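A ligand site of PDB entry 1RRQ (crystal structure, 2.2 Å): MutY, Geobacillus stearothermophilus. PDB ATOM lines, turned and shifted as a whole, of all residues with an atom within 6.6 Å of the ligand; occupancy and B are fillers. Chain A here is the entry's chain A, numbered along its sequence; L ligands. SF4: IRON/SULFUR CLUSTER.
SG of Cys 211 sits close to N of Val 213 (3.5 Å).
O of Leu 157 is in hydrogen-bond range of N of Gln 218.
The backbone carbonyl oxygen of Ala 219 sits at hydrogen-bond distance from the backbone NH of Ala 225 (3.1 Å).
The side-chain sulfur of Cys 217 lies close to the backbone NH of Phe 220, at 3.5 Å.
The side-chain amide nitrogen (NE2) of Gln 214 is in hydrogen-bond range of the backbone carbonyl oxygen (O) of Cys 208 (2.7 Å).
The side-chain sulfur (SG) of Cys 217 sits close to the backbone carbonyl oxygen (O) of Arg 156.
O of Val 200 is in hydrogen-bond range of N of Ser 207, at 3.1 Å.
The backbone carbonyl oxygen (O) of Leu 196 is in hydrogen-bond range of the backbone NH (N) of Cys 201 (2.9 Å).
Merely in contact with the ligand: Ala 225, Arg 156, Leu 157 and Val 200.
Hydrophobic or aromatic side chains that line the ligand: Leu 157, Val 200 and Ala 225.
Within 4 Å of the ligand: Arg 156, Leu 157, Val 200, Cys 201, Cys 208, Cys 211, Cys 217 and Ala 225.
The nearest printed residue that does not touch the ligand is Val 213 (4.03 Å).
The side-chain sulfur (SG) of Cys 208 is bound to an iron atom (FE3) of the ligand, at 2.3 Å.
An iron atom (FE2) of the ligand is bound by the side-chain sulfur (SG) of Cys 201 (2.5 Å).
SG of Cys 211 is bound to FE1 of the ligand.
SG of Cys 217 binds FE4 of the ligand (2.5 Å).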
ATOM      1  N   ARG A 152       7.914 -25.896  28.131  1.00  0.00           N
ATOM      2  CA  ARG A 152       7.322 -25.076  27.080  1.00  0.00           C
ATOM      3  C   ARG A 152       6.174 -25.838  26.417  1.00  0.00           C
ATOM      4  O   ARG A 152       5.105 -25.281  26.157  1.00  0.00           O
ATOM      5  CB  ARG A 152       8.348 -24.720  26.016  1.00  0.00           C
ATOM      6  CG  ARG A 152       7.742 -23.968  24.840  1.00  0.00           C
ATOM      7  CD  ARG A 152       8.795 -23.478  23.856  1.00  0.00           C
ATOM      8  NE  ARG A 152       9.519 -24.559  23.185  1.00  0.00           N
ATOM      9  CZ  ARG A 152      10.798 -24.857  23.406  1.00  0.00           C
ATOM     10  NH1 ARG A 152      11.486 -24.151  24.293  1.00  0.00           N
ATOM     11  NH2 ARG A 152      11.391 -25.834  22.729  1.00  0.00           N
ATOM     12  N   VAL A 153       6.399 -27.112  26.146  1.00  0.00           N
ATOM     13  CA  VAL A 153       5.390 -27.936  25.504  1.00  0.00           C
ATOM     14  C   VAL A 153       4.154 -28.147  26.394  1.00  0.00           C
ATOM     15  O   VAL A 153       3.040 -27.880  25.971  1.00  0.00           O
ATOM     16  CB  VAL A 153       5.978 -29.313  25.093  1.00  0.00           C
ATOM     17  CG1 VAL A 153       4.884 -30.193  24.509  1.00  0.00           C
ATOM     18  CG2 VAL A 153       7.076 -29.112  24.048  1.00  0.00           C
ATOM     19  N   ARG A 156       1.750 -25.321  27.167  1.00  0.00           N
ATOM     20  CA  ARG A 156       0.870 -24.997  26.056  1.00  0.00           C
ATOM     21  C   ARG A 156      -0.224 -26.035  25.947  1.00  0.00           C
ATOM     22  O   ARG A 156      -1.404 -25.699  25.826  1.00  0.00           O
ATOM     23  CB  ARG A 156       1.666 -24.923  24.759  1.00  0.00           C
ATOM     24  CG  ARG A 156       2.529 -23.681  24.648  1.00  0.00           C
ATOM     25  CD  ARG A 156       3.487 -23.761  23.473  1.00  0.00           C
ATOM     26  NE  ARG A 156       4.273 -22.543  23.344  1.00  0.00           N
ATOM     27  CZ  ARG A 156       5.270 -22.378  22.476  1.00  0.00           C
ATOM     28  NH1 ARG A 156       5.604 -23.375  21.661  1.00  0.00           N
ATOM     29  NH2 ARG A 156       5.914 -21.224  22.414  1.00  0.00           N
ATOM     30  N   LEU A 157       0.143 -27.313  26.018  1.00  0.00           N
ATOM     31  CA  LEU A 157      -0.854 -28.360  25.941  1.00  0.00           C
ATOM     32  C   LEU A 157      -1.891 -28.224  27.048  1.00  0.00           C
ATOM     33  O   LEU A 157      -3.074 -28.487  26.838  1.00  0.00           O
ATOM     34  CB  LEU A 157      -0.181 -29.733  26.048  1.00  0.00           C
ATOM     35  CG  LEU A 157       0.564 -30.238  24.812  1.00  0.00           C
ATOM     36  CD1 LEU A 157       1.237 -31.549  25.131  1.00  0.00           C
ATOM     37  CD2 LEU A 157      -0.403 -30.388  23.646  1.00  0.00           C
ATOM     38  N   LEU A 196       9.521 -32.808  19.998  1.00  0.00           N
ATOM     39  CA  LEU A 196       8.391 -31.960  19.638  1.00  0.00           C
ATOM     40  C   LEU A 196       8.787 -30.531  19.916  1.00  0.00           C
ATOM     41  O   LEU A 196       8.750 -29.667  19.038  1.00  0.00           O
ATOM     42  CB  LEU A 196       7.135 -32.321  20.464  1.00  0.00           C
ATOM     43  CG  LEU A 196       5.806 -31.688  20.019  1.00  0.00           C
ATOM     44  CD1 LEU A 196       5.347 -32.316  18.702  1.00  0.00           C
ATOM     45  CD2 LEU A 196       4.720 -31.899  21.079  1.00  0.00           C
ATOM     46  N   VAL A 200       8.722 -28.876  16.435  1.00  0.00           N
ATOM     47  CA  VAL A 200       7.402 -28.317  16.200  1.00  0.00           C
ATOM     48  C   VAL A 200       7.003 -27.203  17.159  1.00  0.00           C
ATOM     49  O   VAL A 200       6.900 -26.044  16.766  1.00  0.00           O
ATOM     50  CB  VAL A 200       6.332 -29.450  16.288  1.00  0.00           C
ATOM     51  CG1 VAL A 200       4.947 -28.917  15.973  1.00  0.00           C
ATOM     52  CG2 VAL A 200       6.716 -30.577  15.333  1.00  0.00           C
ATOM     53  N   CYS A 201       6.784 -27.568  18.412  1.00  0.00           N
ATOM     54  CA  CYS A 201       6.382 -26.617  19.442  1.00  0.00           C
ATOM     55  C   CYS A 201       7.593 -25.835  19.943  1.00  0.00           C
ATOM     56  O   CYS A 201       8.006 -25.931  21.108  1.00  0.00           O
ATOM     57  CB  CYS A 201       5.720 -27.390  20.580  1.00  0.00           C
ATOM     58  SG  CYS A 201       5.001 -26.329  21.794  1.00  0.00           S
ATOM     59  N   THR A 202       8.145 -25.022  19.039  1.00  0.00           N
ATOM     60  CA  THR A 202       9.334 -24.226  19.287  1.00  0.00           C
ATOM     61  C   THR A 202       9.106 -22.958  20.116  1.00  0.00           C
ATOM     62  O   THR A 202       7.972 -22.504  20.264  1.00  0.00           O
ATOM     63  CB  THR A 202       9.960 -23.834  17.924  1.00  0.00           C
ATOM     64  OG1 THR A 202       8.987 -23.116  17.152  1.00  0.00           O
ATOM     65  CG2 THR A 202      10.376 -25.074  17.141  1.00  0.00           C
ATOM     66  N   PRO A 206       5.549 -21.497  16.997  1.00  0.00           N
ATOM     67  CA  PRO A 206       5.278 -22.942  17.000  1.00  0.00           C
ATOM     68  C   PRO A 206       4.434 -23.344  15.786  1.00  0.00           C
ATOM     69  O   PRO A 206       3.492 -22.638  15.417  1.00  0.00           O
ATOM     70  CB  PRO A 206       4.581 -23.165  18.338  1.00  0.00           C
ATOM     71  CG  PRO A 206       3.918 -21.850  18.606  1.00  0.00           C
ATOM     72  CD  PRO A 206       4.982 -20.851  18.193  1.00  0.00           C
ATOM     73  N   SER A 207       4.763 -24.465  15.166  1.00  0.00           N
ATOM     74  CA  SER A 207       4.042 -24.937  13.987  1.00  0.00           C
ATOM     75  C   SER A 207       2.838 -25.792  14.337  1.00  0.00           C
ATOM     76  O   SER A 207       2.746 -26.945  13.914  1.00  0.00           O
ATOM     77  CB  SER A 207       4.994 -25.714  13.070  1.00  0.00           C
ATOM     78  OG  SER A 207       6.112 -24.899  12.718  1.00  0.00           O
ATOM     79  N   CYS A 208       1.928 -25.201  15.102  1.00  0.00           N
ATOM     80  CA  CYS A 208       0.720 -25.879  15.568  1.00  0.00           C
ATOM     81  C   CYS A 208      -0.084 -26.574  14.466  1.00  0.00           C
ATOM     82  O   CYS A 208      -0.581 -27.686  14.661  1.00  0.00           O
ATOM     83  CB  CYS A 208      -0.172 -24.855  16.281  1.00  0.00           C
ATOM     84  SG  CYS A 208       0.682 -23.824  17.508  1.00  0.00           S
ATOM     85  N   LEU A 209      -0.206 -25.940  13.314  1.00  0.00           N
ATOM     86  CA  LEU A 209      -0.979 -26.515  12.212  1.00  0.00           C
ATOM     87  C   LEU A 209      -0.476 -27.881  11.716  1.00  0.00           C
ATOM     88  O   LEU A 209      -1.238 -28.635  11.119  1.00  0.00           O
ATOM     89  CB  LEU A 209      -1.024 -25.524  11.040  1.00  0.00           C
ATOM     90  CG  LEU A 209      -1.614 -24.151  11.378  1.00  0.00           C
ATOM     91  CD1 LEU A 209      -1.600 -23.262  10.141  1.00  0.00           C
ATOM     92  CD2 LEU A 209      -3.023 -24.314  11.896  1.00  0.00           C
ATOM     93  N   CYS A 211       1.336 -29.839  13.936  1.00  0.00           N
ATOM     94  CA  CYS A 211       1.626 -30.531  15.185  1.00  0.00           C
ATOM     95  C   CYS A 211       0.809 -31.801  15.331  1.00  0.00           C
ATOM     96  O   CYS A 211      -0.401 -31.799  15.117  1.00  0.00           O
ATOM     97  CB  CYS A 211       1.365 -29.601  16.382  1.00  0.00           C
ATOM     98  SG  CYS A 211       1.687 -30.366  17.992  1.00  0.00           S
ATOM     99  N   PRO A 212       1.462 -32.917  15.704  1.00  0.00           N
ATOM    100  CA  PRO A 212       0.812 -34.216  15.883  1.00  0.00           C
ATOM    101  C   PRO A 212      -0.146 -34.319  17.073  1.00  0.00           C
ATOM    102  O   PRO A 212      -0.960 -35.243  17.134  1.00  0.00           O
ATOM    103  CB  PRO A 212       1.987 -35.168  16.008  1.00  0.00           C
ATOM    104  CG  PRO A 212       3.012 -34.311  16.724  1.00  0.00           C
ATOM    105  CD  PRO A 212       2.913 -33.009  15.979  1.00  0.00           C
ATOM    106  N   VAL A 213      -0.046 -33.397  18.021  1.00  0.00           N
ATOM    107  CA  VAL A 213      -0.901 -33.437  19.194  1.00  0.00           C
ATOM    108  C   VAL A 213      -1.726 -32.159  19.336  1.00  0.00           C
ATOM    109  O   VAL A 213      -2.123 -31.770  20.436  1.00  0.00           O
ATOM    110  CB  VAL A 213      -0.075 -33.647  20.484  1.00  0.00           C
ATOM    111  CG1 VAL A 213       0.763 -34.906  20.356  1.00  0.00           C
ATOM    112  CG2 VAL A 213       0.822 -32.439  20.719  1.00  0.00           C
ATOM    113  N   GLN A 214      -1.977 -31.507  18.212  1.00  0.00           N
ATOM    114  CA  GLN A 214      -2.749 -30.272  18.203  1.00  0.00           C
ATOM    115  C   GLN A 214      -4.139 -30.512  18.804  1.00  0.00           C
ATOM    116  O   GLN A 214      -4.628 -29.727  19.612  1.00  0.00           O
ATOM    117  CB  GLN A 214      -2.888 -29.774  16.780  1.00  0.00           C
ATOM    118  CG  GLN A 214      -3.541 -28.428  16.664  1.00  0.00           C
ATOM    119  CD  GLN A 214      -3.898 -28.100  15.235  1.00  0.00           C
ATOM    120  OE1 GLN A 214      -4.791 -28.713  14.651  1.00  0.00           O
ATOM    121  NE2 GLN A 214      -3.197 -27.131  14.658  1.00  0.00           N
ATOM    122  N   ALA A 215      -4.756 -31.615  18.389  1.00  0.00           N
ATOM    123  CA  ALA A 215      -6.083 -31.978  18.869  1.00  0.00           C
ATOM    124  C   ALA A 215      -6.188 -31.887  20.378  1.00  0.00           C
ATOM    125  O   ALA A 215      -7.267 -31.604  20.914  1.00  0.00           O
ATOM    126  CB  ALA A 215      -6.435 -33.390  18.395  1.00  0.00           C
ATOM    127  N   TYR A 216      -5.081 -32.127  21.078  1.00  0.00           N
ATOM    128  CA  TYR A 216      -5.092 -32.100  22.531  1.00  0.00           C
ATOM    129  C   TYR A 216      -4.553 -30.796  23.112  1.00  0.00           C
ATOM    130  O   TYR A 216      -4.350 -30.711  24.324  1.00  0.00           O
ATOM    131  CB  TYR A 216      -4.243 -33.227  23.115  1.00  0.00           C
ATOM    132  CG  TYR A 216      -4.411 -34.599  22.489  1.00  0.00           C
ATOM    133  CD1 TYR A 216      -3.979 -34.842  21.177  1.00  0.00           C
ATOM    134  CD2 TYR A 216      -4.928 -35.659  23.220  1.00  0.00           C
ATOM    135  CE1 TYR A 216      -4.059 -36.123  20.631  1.00  0.00           C
ATOM    136  CE2 TYR A 216      -5.002 -36.943  22.686  1.00  0.00           C
ATOM    137  CZ  TYR A 216      -4.563 -37.172  21.390  1.00  0.00           C
ATOM    138  OH  TYR A 216      -4.609 -38.441  20.863  1.00  0.00           O
ATOM    139  N   CYS A 217      -4.335 -29.775  22.290  1.00  0.00           N
ATOM    140  CA  CYS A 217      -3.753 -28.546  22.837  1.00  0.00           C
ATOM    141  C   CYS A 217      -4.664 -27.379  23.218  1.00  0.00           C
ATOM    142  O   CYS A 217      -5.301 -26.762  22.368  1.00  0.00           O
ATOM    143  CB  CYS A 217      -2.667 -28.020  21.895  1.00  0.00           C
ATOM    144  SG  CYS A 217      -1.755 -26.656  22.619  1.00  0.00           S
ATOM    145  N   GLN A 218      -4.667 -27.047  24.516  1.00  0.00           N
ATOM    146  CA  GLN A 218      -5.465 -25.952  25.049  1.00  0.00           C
ATOM    147  C   GLN A 218      -4.970 -24.575  24.627  1.00  0.00           C
ATOM    148  O   GLN A 218      -5.763 -23.652  24.422  1.00  0.00           O
ATOM    149  CB  GLN A 218      -5.483 -25.987  26.578  1.00  0.00           C
ATOM    150  CG  GLN A 218      -6.402 -27.018  27.195  1.00  0.00           C
ATOM    151  CD  GLN A 218      -6.414 -26.910  28.703  1.00  0.00           C
ATOM    152  OE1 GLN A 218      -6.583 -25.821  29.261  1.00  0.00           O
ATOM    153  NE2 GLN A 218      -6.241 -28.052  29.384  1.00  0.00           N
ATOM    154  N   ALA A 219      -3.658 -24.430  24.515  1.00  0.00           N
ATOM    155  CA  ALA A 219      -3.085 -23.145  24.143  1.00  0.00           C
ATOM    156  C   ALA A 219      -3.448 -22.797  22.707  1.00  0.00           C
ATOM    157  O   ALA A 219      -3.590 -21.630  22.350  1.00  0.00           O
ATOM    158  CB  ALA A 219      -1.566 -23.160  24.308  1.00  0.00           C
ATOM    159  N   PHE A 220      -3.596 -23.820  21.867  1.00  0.00           N
ATOM    160  CA  PHE A 220      -3.952 -23.591  20.476  1.00  0.00           C
ATOM    161  C   PHE A 220      -5.426 -23.243  20.404  1.00  0.00           C
ATOM    162  O   PHE A 220      -5.812 -22.285  19.744  1.00  0.00           O
ATOM    163  CB  PHE A 220      -3.671 -24.834  19.620  1.00  0.00           C
ATOM    164  CG  PHE A 220      -3.973 -24.642  18.159  1.00  0.00           C
ATOM    165  CD1 PHE A 220      -3.402 -23.590  17.457  1.00  0.00           C
ATOM    166  CD2 PHE A 220      -4.826 -25.513  17.493  1.00  0.00           C
ATOM    167  CE1 PHE A 220      -3.676 -23.401  16.096  1.00  0.00           C
ATOM    168  CE2 PHE A 220      -5.107 -25.330  16.134  1.00  0.00           C
ATOM    169  CZ  PHE A 220      -4.529 -24.269  15.439  1.00  0.00           C
ATOM    170  N   ALA A 225      -0.918 -20.126  22.258  1.00  0.00           N
ATOM    171  CA  ALA A 225       0.266 -20.958  22.135  1.00  0.00           C
ATOM    172  C   ALA A 225       1.563 -20.176  22.011  1.00  0.00           C
ATOM    173  O   ALA A 225       2.611 -20.614  22.492  1.00  0.00           O
ATOM    174  CB  ALA A 225       0.123 -21.888  20.931  1.00  0.00           C
ATOM    175  N   GLU A 226       1.493 -19.014  21.383  1.00  0.00           N
ATOM    176  CA  GLU A 226       2.677 -18.186  21.181  1.00  0.00           C
ATOM    177  C   GLU A 226       3.032 -17.237  22.329  1.00  0.00           C
ATOM    178  O   GLU A 226       4.069 -16.579  22.297  1.00  0.00           O
ATOM    179  CB  GLU A 226       2.494 -17.399  19.883  1.00  0.00           C
ATOM    180  CG  GLU A 226       3.688 -16.600  19.457  1.00  0.00           C
ATOM    181  CD  GLU A 226       3.491 -16.023  18.075  1.00  0.00           C
ATOM    182  OE1 GLU A 226       3.345 -16.817  17.119  1.00  0.00           O
ATOM    183  OE2 GLU A 226       3.489 -14.781  17.946  1.00  0.00           O
HETATM  184 FE1  SF4 L   1       1.364 -28.306  19.076  1.00  0.00          FE
HETATM  185 FE2  SF4 L   1       2.765 -26.791  20.826  1.00  0.00          FE
HETATM  186 FE3  SF4 L   1       1.144 -25.677  18.825  1.00  0.00          FE
HETATM  187 FE4  SF4 L   1       0.180 -26.809  21.015  1.00  0.00          FE
HETATM  188  S1  SF4 L   1       1.398 -24.950  20.957  1.00  0.00           S
HETATM  189  S2  SF4 L   1      -0.354 -27.040  18.937  1.00  0.00           S
HETATM  190  S3  SF4 L   1       1.650 -28.554  21.411  1.00  0.00           S
HETATM  191  S4  SF4 L   1       2.935 -26.890  18.523  1.00  0.00           S
